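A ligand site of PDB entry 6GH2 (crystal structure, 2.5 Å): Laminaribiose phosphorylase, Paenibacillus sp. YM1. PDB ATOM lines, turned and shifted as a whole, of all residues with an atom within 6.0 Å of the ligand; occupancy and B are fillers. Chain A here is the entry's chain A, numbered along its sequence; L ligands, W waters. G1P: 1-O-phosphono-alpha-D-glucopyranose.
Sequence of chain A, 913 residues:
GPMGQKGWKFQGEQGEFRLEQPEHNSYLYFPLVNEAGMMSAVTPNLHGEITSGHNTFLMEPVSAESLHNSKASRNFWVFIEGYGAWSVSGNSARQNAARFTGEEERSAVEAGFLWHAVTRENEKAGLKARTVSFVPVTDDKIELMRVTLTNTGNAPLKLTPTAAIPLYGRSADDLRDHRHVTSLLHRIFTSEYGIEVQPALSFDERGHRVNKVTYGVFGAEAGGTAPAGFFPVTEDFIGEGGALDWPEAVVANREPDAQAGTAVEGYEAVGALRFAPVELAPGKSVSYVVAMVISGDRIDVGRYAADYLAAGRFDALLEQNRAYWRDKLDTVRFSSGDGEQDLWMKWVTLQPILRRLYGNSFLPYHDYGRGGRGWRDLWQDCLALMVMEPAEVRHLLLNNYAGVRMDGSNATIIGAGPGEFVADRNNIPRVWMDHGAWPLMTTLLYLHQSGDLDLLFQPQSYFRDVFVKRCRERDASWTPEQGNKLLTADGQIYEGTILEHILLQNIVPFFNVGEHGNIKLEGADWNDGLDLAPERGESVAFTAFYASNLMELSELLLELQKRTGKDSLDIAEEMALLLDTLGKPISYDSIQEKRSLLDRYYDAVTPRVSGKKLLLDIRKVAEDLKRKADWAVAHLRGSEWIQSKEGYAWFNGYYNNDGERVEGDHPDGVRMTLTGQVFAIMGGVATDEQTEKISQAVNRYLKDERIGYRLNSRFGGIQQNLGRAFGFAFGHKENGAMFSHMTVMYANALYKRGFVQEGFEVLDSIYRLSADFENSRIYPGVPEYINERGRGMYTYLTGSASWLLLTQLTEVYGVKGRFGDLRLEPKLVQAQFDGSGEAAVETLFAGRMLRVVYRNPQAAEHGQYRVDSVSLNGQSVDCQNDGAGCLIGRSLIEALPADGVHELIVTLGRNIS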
ATOM      1  N   ARG A 355       0.246 -28.526 -24.793  1.00  0.00           N
ATOM      2  CA  ARG A 355      -1.147 -28.932 -24.698  1.00  0.00           C
ATOM      3  C   ARG A 355      -1.750 -29.223 -26.078  1.00  0.00           C
ATOM      4  O   ARG A 355      -2.478 -30.213 -26.232  1.00  0.00           O
ATOM      5  CB  ARG A 355      -1.989 -27.918 -23.947  1.00  0.00           C
ATOM      6  CG  ARG A 355      -3.325 -28.460 -23.490  1.00  0.00           C
ATOM      7  CD  ARG A 355      -4.221 -27.373 -22.924  1.00  0.00           C
ATOM      8  NE  ARG A 355      -5.590 -27.862 -22.703  1.00  0.00           N
ATOM      9  CZ  ARG A 355      -6.118 -28.308 -21.557  1.00  0.00           C
ATOM     10  NH1 ARG A 355      -5.405 -28.368 -20.438  1.00  0.00           N
ATOM     11  NH2 ARG A 355      -7.385 -28.688 -21.542  1.00  0.00           N
ATOM     12  N   ASN A 360      -3.705 -32.707 -24.561  1.00  0.00           N
ATOM     13  CA  ASN A 360      -3.950 -32.848 -23.122  1.00  0.00           C
ATOM     14  C   ASN A 360      -3.895 -34.313 -22.625  1.00  0.00           C
ATOM     15  O   ASN A 360      -4.648 -34.691 -21.720  1.00  0.00           O
ATOM     16  CB  ASN A 360      -5.302 -32.212 -22.794  1.00  0.00           C
ATOM     17  CG  ASN A 360      -5.421 -31.805 -21.340  1.00  0.00           C
ATOM     18  OD1 ASN A 360      -4.472 -31.332 -20.711  1.00  0.00           O
ATOM     19  ND2 ASN A 360      -6.618 -31.948 -20.810  1.00  0.00           N
ATOM     20  N   HIS A 366      -1.551 -37.645 -16.862  1.00  0.00           N
ATOM     21  CA  HIS A 366      -2.694 -37.537 -17.763  1.00  0.00           C
ATOM     22  C   HIS A 366      -3.004 -38.911 -18.381  1.00  0.00           C
ATOM     23  O   HIS A 366      -2.950 -39.115 -19.570  1.00  0.00           O
ATOM     24  CB  HIS A 366      -2.438 -36.485 -18.878  1.00  0.00           C
ATOM     25  CG  HIS A 366      -2.354 -35.068 -18.387  1.00  0.00           C
ATOM     26  ND1 HIS A 366      -1.254 -34.569 -17.719  1.00  0.00           N
ATOM     27  CD2 HIS A 366      -3.218 -34.031 -18.512  1.00  0.00           C
ATOM     28  CE1 HIS A 366      -1.453 -33.296 -17.447  1.00  0.00           C
ATOM     29  NE2 HIS A 366      -2.640 -32.950 -17.911  1.00  0.00           N
ATOM     30  N   ARG A 376     -13.654 -26.293 -24.911  1.00  0.00           N
ATOM     31  CA  ARG A 376     -12.887 -25.244 -24.237  1.00  0.00           C
ATOM     32  C   ARG A 376     -11.514 -25.013 -24.865  1.00  0.00           C
ATOM     33  O   ARG A 376     -11.042 -23.856 -24.920  1.00  0.00           O
ATOM     34  CB  ARG A 376     -12.680 -25.585 -22.755  1.00  0.00           C
ATOM     35  CG  ARG A 376     -13.958 -25.508 -21.953  1.00  0.00           C
ATOM     36  CD  ARG A 376     -13.730 -25.930 -20.511  1.00  0.00           C
ATOM     37  NE  ARG A 376     -15.007 -26.053 -19.800  1.00  0.00           N
ATOM     38  CZ  ARG A 376     -15.235 -26.884 -18.790  1.00  0.00           C
ATOM     39  NH1 ARG A 376     -14.281 -27.689 -18.333  1.00  0.00           N
ATOM     40  NH2 ARG A 376     -16.423 -26.913 -18.223  1.00  0.00           N
ATOM     41  N   ASP A 377     -10.868 -26.092 -25.310  1.00  0.00           N
ATOM     42  CA  ASP A 377      -9.537 -26.058 -25.913  1.00  0.00           C
ATOM     43  C   ASP A 377      -9.545 -25.253 -27.226  1.00  0.00           C
ATOM     44  O   ASP A 377      -8.577 -24.550 -27.542  1.00  0.00           O
ATOM     45  CB  ASP A 377      -9.004 -27.476 -26.193  1.00  0.00           C
ATOM     46  CG  ASP A 377      -8.879 -28.332 -24.932  1.00  0.00           C
ATOM     47  OD1 ASP A 377      -8.890 -27.815 -23.815  1.00  0.00           O
ATOM     48  OD2 ASP A 377      -8.797 -29.568 -25.070  1.00  0.00           O
ATOM     49  N   GLN A 380      -9.354 -21.788 -25.730  1.00  0.00           N
ATOM     50  CA  GLN A 380      -8.179 -21.556 -24.905  1.00  0.00           C
ATOM     51  C   GLN A 380      -6.902 -21.562 -25.747  1.00  0.00           C
ATOM     52  O   GLN A 380      -6.059 -20.691 -25.560  1.00  0.00           O
ATOM     53  CB  GLN A 380      -8.095 -22.582 -23.783  1.00  0.00           C
ATOM     54  CG  GLN A 380      -7.125 -22.251 -22.664  1.00  0.00           C
ATOM     55  CD  GLN A 380      -7.263 -23.224 -21.520  1.00  0.00           C
ATOM     56  OE1 GLN A 380      -7.735 -22.861 -20.444  1.00  0.00           O
ATOM     57  NE2 GLN A 380      -6.895 -24.487 -21.745  1.00  0.00           N
ATOM     58  N   ASP A 434     -20.949 -23.380 -18.702  1.00  0.00           N
ATOM     59  CA  ASP A 434     -19.919 -22.378 -19.019  1.00  0.00           C
ATOM     60  C   ASP A 434     -19.447 -22.355 -20.464  1.00  0.00           C
ATOM     61  O   ASP A 434     -18.740 -21.426 -20.854  1.00  0.00           O
ATOM     62  CB  ASP A 434     -18.679 -22.588 -18.144  1.00  0.00           C
ATOM     63  CG  ASP A 434     -17.956 -23.878 -18.486  1.00  0.00           C
ATOM     64  OD1 ASP A 434     -18.613 -24.918 -18.380  1.00  0.00           O
ATOM     65  OD2 ASP A 434     -16.760 -23.856 -18.865  1.00  0.00           O
ATOM     66  N   ASP A 525     -20.050 -26.568 -14.578  1.00  0.00           N
ATOM     67  CA  ASP A 525     -19.493 -25.338 -15.157  1.00  0.00           C
ATOM     68  C   ASP A 525     -18.003 -25.596 -15.451  1.00  0.00           C
ATOM     69  O   ASP A 525     -17.645 -26.723 -15.798  1.00  0.00           O
ATOM     70  CB  ASP A 525     -19.785 -24.102 -14.280  1.00  0.00           C
ATOM     71  CG  ASP A 525     -19.194 -24.179 -12.880  1.00  0.00           C
ATOM     72  OD1 ASP A 525     -18.459 -25.146 -12.568  1.00  0.00           O
ATOM     73  OD2 ASP A 525     -19.478 -23.247 -12.091  1.00  0.00           O
ATOM     74  N   TRP A 526     -17.150 -24.573 -15.371  1.00  0.00           N
ATOM     75  CA  TRP A 526     -15.701 -24.755 -15.462  1.00  0.00           C
ATOM     76  C   TRP A 526     -15.235 -25.954 -14.640  1.00  0.00           C
ATOM     77  O   TRP A 526     -14.426 -26.750 -15.105  1.00  0.00           O
ATOM     78  CB  TRP A 526     -14.969 -23.493 -15.000  1.00  0.00           C
ATOM     79  CG  TRP A 526     -13.482 -23.637 -14.886  1.00  0.00           C
ATOM     80  CD1 TRP A 526     -12.563 -23.393 -15.857  1.00  0.00           C
ATOM     81  CD2 TRP A 526     -12.746 -24.068 -13.737  1.00  0.00           C
ATOM     82  NE1 TRP A 526     -11.314 -23.646 -15.395  1.00  0.00           N
ATOM     83  CE2 TRP A 526     -11.384 -24.070 -14.092  1.00  0.00           C
ATOM     84  CE3 TRP A 526     -13.108 -24.469 -12.441  1.00  0.00           C
ATOM     85  CZ2 TRP A 526     -10.373 -24.444 -13.201  1.00  0.00           C
ATOM     86  CZ3 TRP A 526     -12.096 -24.844 -11.549  1.00  0.00           C
ATOM     87  CH2 TRP A 526     -10.744 -24.837 -11.934  1.00  0.00           C
ATOM     88  N   ASN A 527     -15.745 -26.047 -13.410  1.00  0.00           N
ATOM     89  CA  ASN A 527     -15.420 -27.159 -12.540  1.00  0.00           C
ATOM     90  C   ASN A 527     -16.108 -28.447 -13.041  1.00  0.00           C
ATOM     91  O   ASN A 527     -17.300 -28.653 -12.819  1.00  0.00           O
ATOM     92  CB  ASN A 527     -15.783 -26.834 -11.097  1.00  0.00           C
ATOM     93  CG  ASN A 527     -15.232 -27.843 -10.101  1.00  0.00           C
ATOM     94  OD1 ASN A 527     -15.045 -29.041 -10.405  1.00  0.00           O
ATOM     95  ND2 ASN A 527     -14.994 -27.384  -8.879  1.00  0.00           N
ATOM     96  N   ASP A 528     -15.341 -29.297 -13.707  1.00  0.00           N
ATOM     97  CA  ASP A 528     -15.835 -30.587 -14.220  1.00  0.00           C
ATOM     98  C   ASP A 528     -16.368 -31.513 -13.124  1.00  0.00           C
ATOM     99  O   ASP A 528     -17.155 -32.419 -13.413  1.00  0.00           O
ATOM    100  CB  ASP A 528     -14.729 -31.354 -14.984  1.00  0.00           C
ATOM    101  CG  ASP A 528     -14.338 -30.692 -16.306  1.00  0.00           C
ATOM    102  OD1 ASP A 528     -15.026 -29.741 -16.796  1.00  0.00           O
ATOM    103  OD2 ASP A 528     -13.320 -31.186 -16.850  1.00  0.00           O
ATOM    104  N   GLY A 529     -15.892 -31.311 -11.892  1.00  0.00           N
ATOM    105  CA  GLY A 529     -16.305 -32.092 -10.735  1.00  0.00           C
ATOM    106  C   GLY A 529     -17.629 -31.724 -10.113  1.00  0.00           C
ATOM    107  O   GLY A 529     -18.092 -32.456  -9.225  1.00  0.00           O
ATOM    108  N   LYS A 733      -6.981 -32.050  -6.793  1.00  0.00           N
ATOM    109  CA  LYS A 733      -7.794 -31.885  -8.002  1.00  0.00           C
ATOM    110  C   LYS A 733      -8.807 -30.764  -7.737  1.00  0.00           C
ATOM    111  O   LYS A 733      -8.417 -29.754  -7.178  1.00  0.00           O
ATOM    112  CB  LYS A 733      -8.405 -33.237  -8.452  1.00  0.00           C
ATOM    113  CG  LYS A 733      -7.584 -33.992  -9.482  1.00  0.00           C
ATOM    114  CD  LYS A 733      -7.821 -33.441 -10.894  1.00  0.00           C
ATOM    115  CE  LYS A 733      -6.953 -34.158 -11.945  1.00  0.00           C
ATOM    116  NZ  LYS A 733      -6.999 -33.502 -13.292  1.00  0.00           N
ATOM    117  N   GLU A 734     -10.085 -30.942  -8.058  1.00  0.00           N
ATOM    118  CA  GLU A 734     -11.035 -29.846  -7.905  1.00  0.00           C
ATOM    119  C   GLU A 734     -11.626 -29.735  -6.481  1.00  0.00           C
ATOM    120  O   GLU A 734     -12.511 -28.898  -6.266  1.00  0.00           O
ATOM    121  CB  GLU A 734     -12.145 -29.993  -8.949  1.00  0.00           C
ATOM    122  CG  GLU A 734     -11.672 -29.825 -10.396  1.00  0.00           C
ATOM    123  CD  GLU A 734     -11.303 -31.118 -11.101  1.00  0.00           C
ATOM    124  OE1 GLU A 734     -11.066 -32.146 -10.405  1.00  0.00           O
ATOM    125  OE2 GLU A 734     -11.265 -31.084 -12.363  1.00  0.00           O
ATOM    126  N   PHE A 739      -5.651 -24.810  -7.422  1.00  0.00           N
ATOM    127  CA  PHE A 739      -5.896 -25.181  -8.788  1.00  0.00           C
ATOM    128  C   PHE A 739      -5.509 -24.015  -9.687  1.00  0.00           C
ATOM    129  O   PHE A 739      -6.238 -23.024  -9.816  1.00  0.00           O
ATOM    130  CB  PHE A 739      -7.345 -25.586  -8.968  1.00  0.00           C
ATOM    131  CG  PHE A 739      -7.556 -26.567 -10.099  1.00  0.00           C
ATOM    132  CD1 PHE A 739      -7.597 -26.120 -11.427  1.00  0.00           C
ATOM    133  CD2 PHE A 739      -7.716 -27.928  -9.836  1.00  0.00           C
ATOM    134  CE1 PHE A 739      -7.791 -27.007 -12.461  1.00  0.00           C
ATOM    135  CE2 PHE A 739      -7.912 -28.817 -10.884  1.00  0.00           C
ATOM    136  CZ  PHE A 739      -7.943 -28.358 -12.193  1.00  0.00           C
ATOM    137  N   SER A 740      -4.338 -24.154 -10.326  1.00  0.00           N
ATOM    138  CA  SER A 740      -3.626 -23.042 -10.943  1.00  0.00           C
ATOM    139  C   SER A 740      -4.467 -22.178 -11.867  1.00  0.00           C
ATOM    140  O   SER A 740      -4.316 -20.973 -11.871  1.00  0.00           O
ATOM    141  CB  SER A 740      -2.408 -23.552 -11.707  1.00  0.00           C
ATOM    142  OG  SER A 740      -1.478 -24.149 -10.818  1.00  0.00           O
ATOM    143  N   HIS A 741      -5.346 -22.809 -12.653  1.00  0.00           N
ATOM    144  CA  HIS A 741      -6.124 -22.105 -13.667  1.00  0.00           C
ATOM    145  C   HIS A 741      -7.056 -21.085 -13.027  1.00  0.00           C
ATOM    146  O   HIS A 741      -7.083 -19.911 -13.429  1.00  0.00           O
ATOM    147  CB  HIS A 741      -6.944 -23.112 -14.471  1.00  0.00           C
ATOM    148  CG  HIS A 741      -7.618 -22.525 -15.669  1.00  0.00           C
ATOM    149  ND1 HIS A 741      -8.302 -23.307 -16.572  1.00  0.00           N
ATOM    150  CD2 HIS A 741      -7.682 -21.259 -16.145  1.00  0.00           C
ATOM    151  CE1 HIS A 741      -8.795 -22.545 -17.521  1.00  0.00           C
ATOM    152  NE2 HIS A 741      -8.438 -21.303 -17.292  1.00  0.00           N
ATOM    153  N   GLU A 784      -0.988 -28.144 -13.094  1.00  0.00           N
ATOM    154  CA  GLU A 784      -2.449 -28.023 -12.962  1.00  0.00           C
ATOM    155  C   GLU A 784      -2.855 -27.679 -11.537  1.00  0.00           C
ATOM    156  O   GLU A 784      -3.697 -26.809 -11.319  1.00  0.00           O
ATOM    157  CB  GLU A 784      -3.133 -29.320 -13.353  1.00  0.00           C
ATOM    158  CG  GLU A 784      -4.649 -29.266 -13.296  1.00  0.00           C
ATOM    159  CD  GLU A 784      -5.268 -30.595 -13.582  1.00  0.00           C
ATOM    160  OE1 GLU A 784      -5.108 -31.536 -12.789  1.00  0.00           O
ATOM    161  OE2 GLU A 784      -5.917 -30.720 -14.614  1.00  0.00           O
ATOM    162  N   TYR A 794       0.018 -32.981 -12.342  1.00  0.00           N
ATOM    163  CA  TYR A 794      -0.463 -32.842 -13.724  1.00  0.00           C
ATOM    164  C   TYR A 794       0.293 -31.706 -14.409  1.00  0.00           C
ATOM    165  O   TYR A 794      -0.234 -30.629 -14.674  1.00  0.00           O
ATOM    166  CB  TYR A 794      -2.006 -32.690 -13.781  1.00  0.00           C
ATOM    167  CG  TYR A 794      -2.740 -33.968 -13.416  1.00  0.00           C
ATOM    168  CD1 TYR A 794      -2.856 -34.348 -12.099  1.00  0.00           C
ATOM    169  CD2 TYR A 794      -3.287 -34.802 -14.380  1.00  0.00           C
ATOM    170  CE1 TYR A 794      -3.502 -35.515 -11.736  1.00  0.00           C
ATOM    171  CE2 TYR A 794      -3.953 -35.978 -14.027  1.00  0.00           C
ATOM    172  CZ  TYR A 794      -4.044 -36.322 -12.683  1.00  0.00           C
ATOM    173  OH  TYR A 794      -4.672 -37.484 -12.273  1.00  0.00           O
ATOM    174  N   LEU A 797       0.705 -29.778 -19.295  1.00  0.00           N
ATOM    175  CA  LEU A 797      -0.420 -29.633 -20.204  1.00  0.00           C
ATOM    176  C   LEU A 797      -1.534 -28.680 -19.723  1.00  0.00           C
ATOM    177  O   LEU A 797      -2.323 -28.207 -20.517  1.00  0.00           O
ATOM    178  CB  LEU A 797      -0.960 -31.019 -20.528  1.00  0.00           C
ATOM    179  CG  LEU A 797       0.108 -32.007 -21.026  1.00  0.00           C
ATOM    180  CD1 LEU A 797      -0.529 -33.351 -21.379  1.00  0.00           C
ATOM    181  CD2 LEU A 797       0.906 -31.501 -22.227  1.00  0.00           C
ATOM    182  N   THR A 798      -1.586 -28.365 -18.430  1.00  0.00           N
ATOM    183  CA  THR A 798      -2.564 -27.410 -17.867  1.00  0.00           C
ATOM    184  C   THR A 798      -2.790 -26.104 -18.646  1.00  0.00           C
ATOM    185  O   THR A 798      -1.835 -25.427 -19.014  1.00  0.00           O
ATOM    186  CB  THR A 798      -2.227 -27.030 -16.407  1.00  0.00           C
ATOM    187  OG1 THR A 798      -3.144 -26.032 -15.946  1.00  0.00           O
ATOM    188  CG2 THR A 798      -0.817 -26.507 -16.256  1.00  0.00           C
ATOM    189  N   GLY A 799      -4.062 -25.762 -18.837  1.00  0.00           N
ATOM    190  CA  GLY A 799      -4.476 -24.493 -19.425  1.00  0.00           C
ATOM    191  C   GLY A 799      -4.125 -23.251 -18.631  1.00  0.00           C
ATOM    192  O   GLY A 799      -4.177 -22.140 -19.170  1.00  0.00           O
ATOM    193  N   SER A 800      -3.769 -23.404 -17.360  1.00  0.00           N
ATOM    194  CA  SER A 800      -3.349 -22.277 -16.535  1.00  0.00           C
ATOM    195  C   SER A 800      -2.173 -21.492 -17.126  1.00  0.00           C
ATOM    196  O   SER A 800      -2.066 -20.289 -16.914  1.00  0.00           O
ATOM    197  CB  SER A 800      -2.989 -22.749 -15.125  1.00  0.00           C
ATOM    198  OG  SER A 800      -1.946 -23.711 -15.160  1.00  0.00           O
HETATM  199  C1  G1P L   1      -8.609 -28.942 -16.106  1.00  0.00           C
HETATM  200  C2  G1P L   1      -9.366 -28.989 -17.425  1.00  0.00           C
HETATM  201  C3  G1P L   1     -10.293 -27.787 -17.562  1.00  0.00           C
HETATM  202  C4  G1P L   1     -11.249 -27.701 -16.379  1.00  0.00           C
HETATM  203  C5  G1P L   1     -10.493 -27.821 -15.047  1.00  0.00           C
HETATM  204  C6  G1P L   1     -11.455 -27.921 -13.862  1.00  0.00           C
HETATM  205  O1  G1P L   1      -7.793 -27.778 -16.001  1.00  0.00           O
HETATM  206  O2  G1P L   1      -8.457 -29.055 -18.532  1.00  0.00           O
HETATM  207  O3  G1P L   1     -11.048 -27.898 -18.770  1.00  0.00           O
HETATM  208  O4  G1P L   1     -11.961 -26.452 -16.438  1.00  0.00           O
HETATM  209  O5  G1P L   1      -9.591 -28.942 -15.051  1.00  0.00           O
HETATM  210  O6  G1P L   1     -12.275 -29.091 -13.943  1.00  0.00           O
HETATM  211  P   G1P L   1      -6.281 -27.612 -16.542  1.00  0.00           P
HETATM  212  O1P G1P L   1      -5.699 -26.646 -15.539  1.00  0.00           O
HETATM  213  O2P G1P L   1      -6.431 -27.016 -17.923  1.00  0.00           O
HETATM  214  O3P G1P L   1      -5.613 -28.955 -16.556  1.00  0.00           O
HETATM  215  O   HOH W   1      -9.552 -32.238 -14.008  1.00  0.00           O
HETATM  216  O   HOH W   2      -3.640 -30.536 -18.282  1.00  0.00           O
HETATM  217  O   HOH W   3      -5.045 -25.480 -13.212  1.00  0.00           O
HETATM  218  O   HOH W   4     -11.311 -30.338 -20.686  1.00  0.00           O
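OE2 of Glu 784 lies close to O3P of the ligand (2.6 Å).
An oxygen (O1P) of the ligand is in hydrogen-bond range of the side-chain hydroxyl (OG1) of Thr 798 (2.7 Å).
O6 of the ligand lies within hydrogen-bond range of OE2 of Glu 734 (2.7 Å).
O4 of the ligand lies within hydrogen-bond range of O of Trp 526, at 2.8 Å.
NE1 of Trp 526 sits at hydrogen-bond distance from O4 of the ligand, 3.1 Å away.
The backbone NH of Gly 799 is in hydrogen-bond range of an oxygen (O2P) of the ligand.
The guanidinium group (NH1) of Arg 355 lies within salt-bridge range of an oxygen (O2P) of the ligand (3.0 Å).
The backbone NH of Asp 528 lies within hydrogen-bond range of an oxygen (O6) of the ligand, 3.1 Å away.
O4 of the ligand sits at hydrogen-bond distance from NH1 of Arg 376.
The backbone carbonyl oxygen of Tyr 794 is in hydrogen-bond range of the backbone NH of Glu 784, at 3.0 Å.
N of Ser 740 is in hydrogen-bond range of O of Glu 784 (2.9 Å).
O of Trp 526 lies within hydrogen-bond range of NH1 of Arg 376.
ND1 of His 741 lies within hydrogen-bond range of NE1 of Trp 526 (3.3 Å).
The side-chain amide oxygen (OD1) of Asn 360 is in hydrogen-bond range of the guanidinium group (NH1) of Arg 355 (3.1 Å).
NH1 of Arg 355 sits at hydrogen-bond distance from O of Leu 797.
The side-chain carboxylate (OD1) of Asp 377 lies within salt-bridge range of the guanidinium group (NH2) of Arg 355 (2.9 Å).
OD1 of Asn 527 is in hydrogen-bond range of N of Gly 529, at 2.8 Å.
Asn 527 touches the ligand.
CZ of Phe 739 touches O5 of the ligand (3.4 Å).
His 741 touches the ligand (CB to O1P, 3.9 Å).
Within 4 Å of the ligand: Arg 355, Arg 376, Trp 526, Asn 527, Asp 528, Glu 734, Phe 739, His 741, Glu 784, Thr 798 and Gly 799.
Along chain A the residues within 4 Å of the ligand span positions 355 to 799.
Water W3 lies within hydrogen-bond range of the backbone carbonyl oxygen (O) of Glu 784 (2.7 Å), an oxygen (O1P) of the ligand (2.7 Å), the backbone NH (N) of His 741 (2.7 Å), the backbone NH (N) of Ser 740 (3.3 Å) and the side-chain hydroxyl (OG1) of Thr 798 (3.4 Å).
Water W2 lies within hydrogen-bond range of NE2 of His 366, OD1 of Asn 360, N of Thr 798, O3P of the ligand and O of Leu 797.
Water W1 lies within hydrogen-bond range of OE2 of Glu 734, NZ of Lys 733 and O5 of the ligand.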
